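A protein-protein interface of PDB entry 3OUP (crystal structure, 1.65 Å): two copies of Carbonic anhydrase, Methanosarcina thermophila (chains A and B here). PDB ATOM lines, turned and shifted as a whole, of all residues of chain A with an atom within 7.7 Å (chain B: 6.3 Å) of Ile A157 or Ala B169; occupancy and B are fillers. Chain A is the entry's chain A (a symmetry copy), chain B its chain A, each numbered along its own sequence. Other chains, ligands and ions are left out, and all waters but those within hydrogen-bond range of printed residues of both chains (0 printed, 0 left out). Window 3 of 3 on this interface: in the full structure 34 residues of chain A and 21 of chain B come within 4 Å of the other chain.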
ATOM      1  N   PHE A 138      11.535 -11.734 -13.013  1.00  0.00           N
ATOM      2  CA  PHE A 138      11.674 -12.487 -11.765  1.00  0.00           C
ATOM      3  C   PHE A 138      12.351 -13.808 -12.104  1.00  0.00           C
ATOM      4  O   PHE A 138      11.964 -14.482 -13.073  1.00  0.00           O
ATOM      5  CB  PHE A 138      10.295 -12.750 -11.156  1.00  0.00           C
ATOM      6  CG  PHE A 138      10.334 -13.570  -9.908  1.00  0.00           C
ATOM      7  CD1 PHE A 138      10.936 -13.069  -8.753  1.00  0.00           C
ATOM      8  CD2 PHE A 138       9.757 -14.824  -9.869  1.00  0.00           C
ATOM      9  CE1 PHE A 138      10.959 -13.815  -7.580  1.00  0.00           C
ATOM     10  CE2 PHE A 138       9.772 -15.566  -8.704  1.00  0.00           C
ATOM     11  CZ  PHE A 138      10.398 -15.079  -7.565  1.00  0.00           C
ATOM     12  N   VAL A 139      13.364 -14.164 -11.326  1.00  0.00           N
ATOM     13  CA  VAL A 139      14.067 -15.449 -11.534  1.00  0.00           C
ATOM     14  C   VAL A 139      14.182 -16.129 -10.173  1.00  0.00           C
ATOM     15  O   VAL A 139      14.650 -15.486  -9.243  1.00  0.00           O
ATOM     16  CB  VAL A 139      15.495 -15.188 -12.058  1.00  0.00           C
ATOM     17  CG1 VAL A 139      16.262 -16.507 -12.157  1.00  0.00           C
ATOM     18  CG2 VAL A 139      15.471 -14.475 -13.422  1.00  0.00           C
ATOM     19  N   PHE A 140      13.763 -17.392 -10.037  1.00  0.00           N
ATOM     20  CA  PHE A 140      13.770 -18.061  -8.724  1.00  0.00           C
ATOM     21  C   PHE A 140      13.918 -19.553  -8.976  1.00  0.00           C
ATOM     22  O   PHE A 140      13.216 -20.088  -9.826  1.00  0.00           O
ATOM     23  CB  PHE A 140      12.434 -17.780  -8.080  1.00  0.00           C
ATOM     24  CG  PHE A 140      12.194 -18.471  -6.754  1.00  0.00           C
ATOM     25  CD1 PHE A 140      13.197 -18.537  -5.782  1.00  0.00           C
ATOM     26  CD2 PHE A 140      10.932 -18.981  -6.462  1.00  0.00           C
ATOM     27  CE1 PHE A 140      12.946 -19.147  -4.529  1.00  0.00           C
ATOM     28  CE2 PHE A 140      10.661 -19.584  -5.219  1.00  0.00           C
ATOM     29  CZ  PHE A 140      11.681 -19.666  -4.248  1.00  0.00           C
ATOM     30  N   LYS A 141      14.816 -20.220  -8.251  1.00  0.00           N
ATOM     31  CA  LYS A 141      15.024 -21.660  -8.433  1.00  0.00           C
ATOM     32  C   LYS A 141      15.281 -21.986  -9.901  1.00  0.00           C
ATOM     33  O   LYS A 141      14.771 -22.967 -10.430  1.00  0.00           O
ATOM     34  CB  LYS A 141      13.799 -22.455  -7.947  1.00  0.00           C
ATOM     35  CG  LYS A 141      13.599 -22.397  -6.445  1.00  0.00           C
ATOM     36  CD  LYS A 141      12.421 -23.276  -6.022  1.00  0.00           C
ATOM     37  CE  LYS A 141      12.469 -23.582  -4.541  1.00  0.00           C
ATOM     38  NZ  LYS A 141      11.372 -24.511  -4.148  1.00  0.00           N
ATOM     39  N   SER A 142      16.102 -21.175 -10.555  1.00  0.00           N
ATOM     40  CA  SER A 142      16.342 -21.356 -11.983  1.00  0.00           C
ATOM     41  C   SER A 142      17.802 -21.090 -12.316  1.00  0.00           C
ATOM     42  O   SER A 142      18.502 -20.345 -11.616  1.00  0.00           O
ATOM     43  CB  SER A 142      15.479 -20.387 -12.823  1.00  0.00           C
ATOM     44  OG  SER A 142      14.098 -20.739 -12.755  1.00  0.00           O
ATOM     45  N   LYS A 143      18.240 -21.693 -13.422  1.00  0.00           N
ATOM     46  CA  LYS A 143      19.519 -21.353 -14.009  1.00  0.00           C
ATOM     47  C   LYS A 143      19.230 -20.727 -15.364  1.00  0.00           C
ATOM     48  O   LYS A 143      18.614 -21.364 -16.222  1.00  0.00           O
ATOM     49  CB  LYS A 143      20.382 -22.610 -14.156  1.00  0.00           C
ATOM     50  CG  LYS A 143      20.707 -23.281 -12.825  1.00  0.00           C
ATOM     51  CD  LYS A 143      21.659 -24.455 -13.007  1.00  0.00           C
ATOM     52  CE  LYS A 143      22.051 -25.082 -11.681  1.00  0.00           C
ATOM     53  NZ  LYS A 143      23.012 -26.203 -11.906  1.00  0.00           N
ATOM     54  N   LEU A 150      15.590 -11.926 -20.745  1.00  0.00           N
ATOM     55  CA  LEU A 150      14.271 -12.039 -20.129  1.00  0.00           C
ATOM     56  C   LEU A 150      13.617 -10.687 -20.419  1.00  0.00           C
ATOM     57  O   LEU A 150      14.077  -9.664 -19.931  1.00  0.00           O
ATOM     58  CB  LEU A 150      14.386 -12.287 -18.602  1.00  0.00           C
ATOM     59  CG  LEU A 150      14.215 -13.788 -18.303  1.00  0.00           C
ATOM     60  CD1 LEU A 150      15.387 -14.573 -18.828  1.00  0.00           C
ATOM     61  CD2 LEU A 150      14.042 -13.997 -16.789  1.00  0.00           C
ATOM     62  N   ALA A 155       9.225 -14.233 -16.352  1.00  0.00           N
ATOM     63  CA  ALA A 155       9.672 -14.898 -15.125  1.00  0.00           C
ATOM     64  C   ALA A 155      10.125 -16.300 -15.463  1.00  0.00           C
ATOM     65  O   ALA A 155       9.577 -16.937 -16.360  1.00  0.00           O
ATOM     66  CB  ALA A 155       8.565 -14.949 -14.090  1.00  0.00           C
ATOM     67  N   ALA A 156      11.134 -16.769 -14.752  1.00  0.00           N
ATOM     68  CA  ALA A 156      11.587 -18.171 -14.876  1.00  0.00           C
ATOM     69  C   ALA A 156      11.611 -18.753 -13.471  1.00  0.00           C
ATOM     70  O   ALA A 156      12.363 -18.276 -12.613  1.00  0.00           O
ATOM     71  CB  ALA A 156      12.968 -18.214 -15.473  1.00  0.00           C
ATOM     72  N   ILE A 157      10.796 -19.780 -13.220  1.00  0.00           N
ATOM     73  CA  ILE A 157      10.726 -20.372 -11.875  1.00  0.00           C
ATOM     74  C   ILE A 157      10.895 -21.878 -12.027  1.00  0.00           C
ATOM     75  O   ILE A 157      10.057 -22.544 -12.669  1.00  0.00           O
ATOM     76  CB  ILE A 157       9.359 -20.108 -11.233  1.00  0.00           C
ATOM     77  CG1 ILE A 157       9.081 -18.583 -11.175  1.00  0.00           C
ATOM     78  CG2 ILE A 157       9.318 -20.691  -9.823  1.00  0.00           C
ATOM     79  CD1 ILE A 157       7.635 -18.242 -10.751  1.00  0.00           C
ATOM     80  N   GLY A 158      11.941 -22.427 -11.420  1.00  0.00           N
ATOM     81  CA  GLY A 158      12.101 -23.878 -11.372  1.00  0.00           C
ATOM     82  C   GLY A 158      12.620 -24.501 -12.657  1.00  0.00           C
ATOM     83  O   GLY A 158      12.421 -25.715 -12.902  1.00  0.00           O
ATOM     84  N   VAL A 159      13.258 -23.703 -13.506  1.00  0.00           N
ATOM     85  CA  VAL A 159      13.690 -24.185 -14.834  1.00  0.00           C
ATOM     86  C   VAL A 159      15.131 -23.830 -15.181  1.00  0.00           C
ATOM     87  O   VAL A 159      15.764 -22.995 -14.524  1.00  0.00           O
ATOM     88  CB  VAL A 159      12.783 -23.635 -15.957  1.00  0.00           C
ATOM     89  CG1 VAL A 159      11.367 -24.134 -15.784  1.00  0.00           C
ATOM     90  CG2 VAL A 159      12.815 -22.089 -15.970  1.00  0.00           C
ATOM     91  N   THR A 160      15.659 -24.506 -16.201  1.00  0.00           N
ATOM     92  CA  THR A 160      16.919 -24.101 -16.789  1.00  0.00           C
ATOM     93  C   THR A 160      16.606 -23.473 -18.148  1.00  0.00           C
ATOM     94  O   THR A 160      15.924 -24.080 -18.982  1.00  0.00           O
ATOM     95  CB  THR A 160      17.844 -25.329 -16.941  1.00  0.00           C
ATOM     96  OG1 THR A 160      18.223 -25.799 -15.639  1.00  0.00           O
ATOM     97  CG2 THR A 160      19.087 -24.999 -17.768  1.00  0.00           C
ATOM     98  N   ILE A 161      17.061 -22.242 -18.368  1.00  0.00           N
ATOM     99  CA  ILE A 161      16.865 -21.558 -19.644  1.00  0.00           C
ATOM    100  C   ILE A 161      18.142 -21.750 -20.455  1.00  0.00           C
ATOM    101  O   ILE A 161      19.224 -21.364 -20.010  1.00  0.00           O
ATOM    102  CB  ILE A 161      16.636 -20.042 -19.442  1.00  0.00           C
ATOM    103  CG1 ILE A 161      15.488 -19.764 -18.432  1.00  0.00           C
ATOM    104  CG2 ILE A 161      16.391 -19.375 -20.786  1.00  0.00           C
ATOM    105  CD1 ILE A 161      14.086 -20.252 -18.897  1.00  0.00           C
ATOM    106  N   ILE A 167      12.775 -14.891 -23.276  1.00  0.00           N
ATOM    107  CA  ILE A 167      11.423 -15.106 -22.812  1.00  0.00           C
ATOM    108  C   ILE A 167      10.633 -13.852 -23.138  1.00  0.00           C
ATOM    109  O   ILE A 167      10.958 -12.768 -22.660  1.00  0.00           O
ATOM    110  CB  ILE A 167      11.344 -15.324 -21.285  1.00  0.00           C
ATOM    111  CG1 ILE A 167      12.257 -16.489 -20.857  1.00  0.00           C
ATOM    112  CG2 ILE A 167       9.893 -15.641 -20.931  1.00  0.00           C
ATOM    113  CD1 ILE A 167      12.160 -16.826 -19.376  1.00  0.00           C
ATOM    114  N   VAL A 172       5.392 -16.310 -18.023  1.00  0.00           N
ATOM    115  CA  VAL A 172       5.886 -16.925 -16.798  1.00  0.00           C
ATOM    116  C   VAL A 172       6.165 -18.394 -17.114  1.00  0.00           C
ATOM    117  O   VAL A 172       5.247 -19.156 -17.442  1.00  0.00           O
ATOM    118  CB  VAL A 172       4.842 -16.814 -15.673  1.00  0.00           C
ATOM    119  CG1 VAL A 172       5.327 -17.534 -14.437  1.00  0.00           C
ATOM    120  CG2 VAL A 172       4.563 -15.349 -15.360  1.00  0.00           C
ATOM    121  N   VAL A 173       7.431 -18.769 -17.063  1.00  0.00           N
ATOM    122  CA  VAL A 173       7.876 -20.100 -17.490  1.00  0.00           C
ATOM    123  C   VAL A 173       8.117 -20.917 -16.226  1.00  0.00           C
ATOM    124  O   VAL A 173       8.967 -20.551 -15.427  1.00  0.00           O
ATOM    125  CB  VAL A 173       9.162 -20.018 -18.330  1.00  0.00           C
ATOM    126  CG1 VAL A 173       9.680 -21.418 -18.740  1.00  0.00           C
ATOM    127  CG2 VAL A 173       8.942 -19.153 -19.575  1.00  0.00           C
ATOM    128  N   THR A 174       7.371 -22.014 -16.053  1.00  0.00           N
ATOM    129  CA  THR A 174       7.476 -22.811 -14.831  1.00  0.00           C
ATOM    130  C   THR A 174       7.736 -24.289 -15.119  1.00  0.00           C
ATOM    131  O   THR A 174       7.826 -25.087 -14.195  1.00  0.00           O
ATOM    132  CB  THR A 174       6.174 -22.757 -13.995  1.00  0.00           C
ATOM    133  OG1 THR A 174       5.072 -23.142 -14.823  1.00  0.00           O
ATOM    134  CG2 THR A 174       5.940 -21.354 -13.427  1.00  0.00           C
ATOM    135  N   SER A 175       7.835 -24.662 -16.384  1.00  0.00           N
ATOM    136  CA  SER A 175       8.059 -26.075 -16.689  1.00  0.00           C
ATOM    137  C   SER A 175       9.189 -26.203 -17.688  1.00  0.00           C
ATOM    138  O   SER A 175       9.347 -25.360 -18.579  1.00  0.00           O
ATOM    139  CB  SER A 175       6.781 -26.743 -17.182  1.00  0.00           C
ATOM    140  OG  SER A 175       6.607 -26.574 -18.567  1.00  0.00           O
ATOM    141  N   GLN A 176       9.998 -27.243 -17.520  1.00  0.00           N
ATOM    142  CA  GLN A 176      11.183 -27.407 -18.342  1.00  0.00           C
ATOM    143  C   GLN A 176      10.797 -27.572 -19.799  1.00  0.00           C
ATOM    144  O   GLN A 176      11.535 -27.154 -20.682  1.00  0.00           O
ATOM    145  CB  GLN A 176      12.024 -28.590 -17.857  1.00  0.00           C
ATOM    146  CG  GLN A 176      13.419 -28.650 -18.463  1.00  0.00           C
ATOM    147  CD  GLN A 176      14.183 -27.349 -18.231  1.00  0.00           C
ATOM    148  OE1 GLN A 176      14.218 -26.849 -17.115  1.00  0.00           O
ATOM    149  NE2 GLN A 176      14.755 -26.788 -19.285  1.00  0.00           N
ATOM    150  N   GLU A 178       8.434 -26.067 -21.426  1.00  0.00           N
ATOM    151  CA  GLU A 178       8.271 -24.717 -21.978  1.00  0.00           C
ATOM    152  C   GLU A 178       9.634 -24.076 -22.242  1.00  0.00           C
ATOM    153  O   GLU A 178       9.846 -23.444 -23.269  1.00  0.00           O
ATOM    154  CB  GLU A 178       7.586 -23.781 -20.984  1.00  0.00           C
ATOM    155  CG  GLU A 178       6.151 -24.051 -20.572  1.00  0.00           C
ATOM    156  CD  GLU A 178       5.626 -22.923 -19.659  1.00  0.00           C
ATOM    157  OE1 GLU A 178       5.064 -21.945 -20.206  1.00  0.00           O
ATOM    158  OE2 GLU A 178       5.805 -22.984 -18.411  1.00  0.00           O
ATOM    159  N   GLU B 151       1.403 -17.675  -4.976  1.00  0.00           N
ATOM    160  CA  GLU B 151       2.732 -17.913  -5.546  1.00  0.00           C
ATOM    161  C   GLU B 151       3.277 -16.619  -6.120  1.00  0.00           C
ATOM    162  O   GLU B 151       2.547 -15.639  -6.326  1.00  0.00           O
ATOM    163  CB  GLU B 151       2.662 -19.001  -6.651  1.00  0.00           C
ATOM    164  CG  GLU B 151       2.381 -20.374  -6.049  1.00  0.00           C
ATOM    165  CD  GLU B 151       2.442 -21.499  -7.073  1.00  0.00           C
ATOM    166  OE1 GLU B 151       2.907 -21.238  -8.194  1.00  0.00           O
ATOM    167  OE2 GLU B 151       2.018 -22.640  -6.744  1.00  0.00           O
ATOM    168  N   PRO B 152       4.567 -16.617  -6.436  1.00  0.00           N
ATOM    169  CA  PRO B 152       5.157 -15.383  -6.982  1.00  0.00           C
ATOM    170  C   PRO B 152       4.382 -14.875  -8.170  1.00  0.00           C
ATOM    171  O   PRO B 152       3.927 -15.685  -9.002  1.00  0.00           O
ATOM    172  CB  PRO B 152       6.577 -15.838  -7.391  1.00  0.00           C
ATOM    173  CG  PRO B 152       6.889 -16.920  -6.395  1.00  0.00           C
ATOM    174  CD  PRO B 152       5.564 -17.682  -6.237  1.00  0.00           C
ATOM    175  N   ARG B 153       4.244 -13.558  -8.266  1.00  0.00           N
ATOM    176  CA  ARG B 153       3.579 -12.907  -9.393  1.00  0.00           C
ATOM    177  C   ARG B 153       2.090 -13.191  -9.528  1.00  0.00           C
ATOM    178  O   ARG B 153       1.517 -12.818 -10.542  1.00  0.00           O
ATOM    179  CB  ARG B 153       4.242 -13.350 -10.701  1.00  0.00           C
ATOM    180  CG  ARG B 153       5.393 -12.536 -11.053  1.00  0.00           C
ATOM    181  CD  ARG B 153       5.005 -11.237 -11.671  1.00  0.00           C
ATOM    182  NE  ARG B 153       6.269 -10.770 -12.167  1.00  0.00           N
ATOM    183  CZ  ARG B 153       6.793 -11.145 -13.320  1.00  0.00           C
ATOM    184  NH1 ARG B 153       6.105 -11.911 -14.186  1.00  0.00           N
ATOM    185  NH2 ARG B 153       7.995 -10.703 -13.616  1.00  0.00           N
ATOM    186  N   SER B 154       1.464 -13.830  -8.534  1.00  0.00           N
ATOM    187  CA  SER B 154      -0.005 -13.963  -8.580  1.00  0.00           C
ATOM    188  C   SER B 154      -0.643 -12.656  -8.060  1.00  0.00           C
ATOM    189  O   SER B 154       0.043 -11.819  -7.501  1.00  0.00           O
ATOM    190  CB  SER B 154      -0.464 -15.144  -7.734  1.00  0.00           C
ATOM    191  OG  SER B 154      -0.106 -14.995  -6.363  1.00  0.00           O
ATOM    192  N   ILE B 167      -2.844 -19.663  -5.218  1.00  0.00           N
ATOM    193  CA  ILE B 167      -2.969 -19.103  -6.545  1.00  0.00           C
ATOM    194  C   ILE B 167      -1.665 -19.378  -7.272  1.00  0.00           C
ATOM    195  O   ILE B 167      -0.605 -18.930  -6.844  1.00  0.00           O
ATOM    196  CB  ILE B 167      -3.181 -17.573  -6.529  1.00  0.00           C
ATOM    197  CG1 ILE B 167      -4.404 -17.205  -5.667  1.00  0.00           C
ATOM    198  CG2 ILE B 167      -3.401 -17.116  -7.969  1.00  0.00           C
ATOM    199  CD1 ILE B 167      -4.732 -15.719  -5.680  1.00  0.00           C
ATOM    200  N   PRO B 168      -1.723 -20.126  -8.375  1.00  0.00           N
ATOM    201  CA  PRO B 168      -0.502 -20.426  -9.131  1.00  0.00           C
ATOM    202  C   PRO B 168       0.227 -19.188  -9.620  1.00  0.00           C
ATOM    203  O   PRO B 168      -0.389 -18.175  -9.943  1.00  0.00           O
ATOM    204  CB  PRO B 168      -1.031 -21.222 -10.344  1.00  0.00           C
ATOM    205  CG  PRO B 168      -2.289 -21.846  -9.841  1.00  0.00           C
ATOM    206  CD  PRO B 168      -2.905 -20.837  -8.911  1.00  0.00           C
ATOM    207  N   ALA B 169       1.542 -19.310  -9.752  1.00  0.00           N
ATOM    208  CA  ALA B 169       2.383 -18.205 -10.200  1.00  0.00           C
ATOM    209  C   ALA B 169       1.832 -17.537 -11.445  1.00  0.00           C
ATOM    210  O   ALA B 169       1.471 -18.210 -12.444  1.00  0.00           O
ATOM    211  CB  ALA B 169       3.806 -18.703 -10.484  1.00  0.00           C
ATOM    212  N   GLY B 170       1.798 -16.207 -11.402  1.00  0.00           N
ATOM    213  CA  GLY B 170       1.405 -15.395 -12.536  1.00  0.00           C
ATOM    214  C   GLY B 170      -0.088 -15.198 -12.740  1.00  0.00           C
ATOM    215  O   GLY B 170      -0.485 -14.358 -13.543  1.00  0.00           O
ATOM    216  N   MET B 171      -0.917 -15.962 -12.026  1.00  0.00           N
ATOM    217  CA  MET B 171      -2.370 -15.877 -12.229  1.00  0.00           C
ATOM    218  C   MET B 171      -2.941 -14.632 -11.554  1.00  0.00           C
ATOM    219  O   MET B 171      -2.638 -14.355 -10.396  1.00  0.00           O
ATOM    220  CB  MET B 171      -3.073 -17.129 -11.699  1.00  0.00           C
ATOM    221  CG  MET B 171      -4.591 -17.130 -11.894  1.00  0.00           C
ATOM    222  SD  MET B 171      -5.348 -18.622 -11.201  1.00  0.00           S
ATOM    223  CE  MET B 171      -4.351 -19.849 -12.039  1.00  0.00           C
ATOM    224  N   TYR B 191       4.672 -25.509  -2.281  1.00  0.00           N
ATOM    225  CA  TYR B 191       4.808 -24.422  -1.289  1.00  0.00           C
ATOM    226  C   TYR B 191       4.073 -24.703   0.030  1.00  0.00           C
ATOM    227  O   TYR B 191       3.832 -23.773   0.812  1.00  0.00           O
ATOM    228  CB  TYR B 191       4.247 -23.104  -1.862  1.00  0.00           C
ATOM    229  CG  TYR B 191       5.022 -22.495  -3.026  1.00  0.00           C
ATOM    230  CD1 TYR B 191       4.806 -22.915  -4.328  1.00  0.00           C
ATOM    231  CD2 TYR B 191       5.928 -21.455  -2.816  1.00  0.00           C
ATOM    232  CE1 TYR B 191       5.496 -22.337  -5.402  1.00  0.00           C
ATOM    233  CE2 TYR B 191       6.613 -20.883  -3.861  1.00  0.00           C
ATOM    234  CZ  TYR B 191       6.403 -21.317  -5.152  1.00  0.00           C
ATOM    235  OH  TYR B 191       7.100 -20.737  -6.192  1.00  0.00           O
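The side-chain carboxylate (OE1) of Glu B151 is in hydrogen-bond range of the backbone NH (N) of Ala B169, at 2.8 Å. The backbone carbonyl oxygen (O) of Ala A155 sits at hydrogen-bond distance from the backbone NH (N) of Val A173 (2.9 Å). The backbone carbonyl oxygen (O) of Phe A140 lies within hydrogen-bond range of the side-chain hydroxyl (OG) of Ser A142. The backbone NH (N) of Phe A140 sits at hydrogen-bond distance from the backbone carbonyl oxygen (O) of Ala A156, at 3.1 Å. The backbone NH (N) of Ala A156 is in hydrogen-bond range of the backbone carbonyl oxygen (O) of Phe A138 (3.0 Å). The backbone carbonyl oxygen (O) of Val A173 lies within hydrogen-bond range of the backbone NH (N) of Ile A157, 3.0 Å away.
Among the printed residues, pairs that only touch across the chains: Phe A138 with Pro B152 (3.5 Å), Phe A138 with Arg B153 (3.7 Å), Phe A140 with Tyr B191 (3.9 Å), Ala A155 with Arg B153 (3.9 Å), Ile A157 with Ala B169 (3.9 Å) and Val A172 with Arg B153 (3.9 Å).
Ile A157 touches just one residue of chain B: Ala B169 (3.9 Å). Ala B169 touches one residue of chain A. Of the printed residues of chain A, Pro B152 touches Phe A138 (3.5 Å). Printed residues of chain B within 4 Å of Ala A155: Arg B153 (3.9 Å). Of the printed residues of chain A, Arg B153 touches Phe A138, Ala A155 and Val A172. Printed residues of chain A within 4 Å of Tyr B191: Phe A140. Ser A175 touches none of the printed residues of chain B. The nearest printed residue of chain B that does not touch Ile A157 is Tyr B191 (4.3 Å). The nearest residue of chain A that does not touch Ala B169 is Val A172 (4.4 Å).
Printed residues of chain B that touch a printed residue of chain A: Pro B152, Arg B153, Ala B169 and Tyr B191.
Position printed for both chains: 167. Of the 6 pairs that touch across the chains among the printed residues, none has its exchanged pair printed and touching as well.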
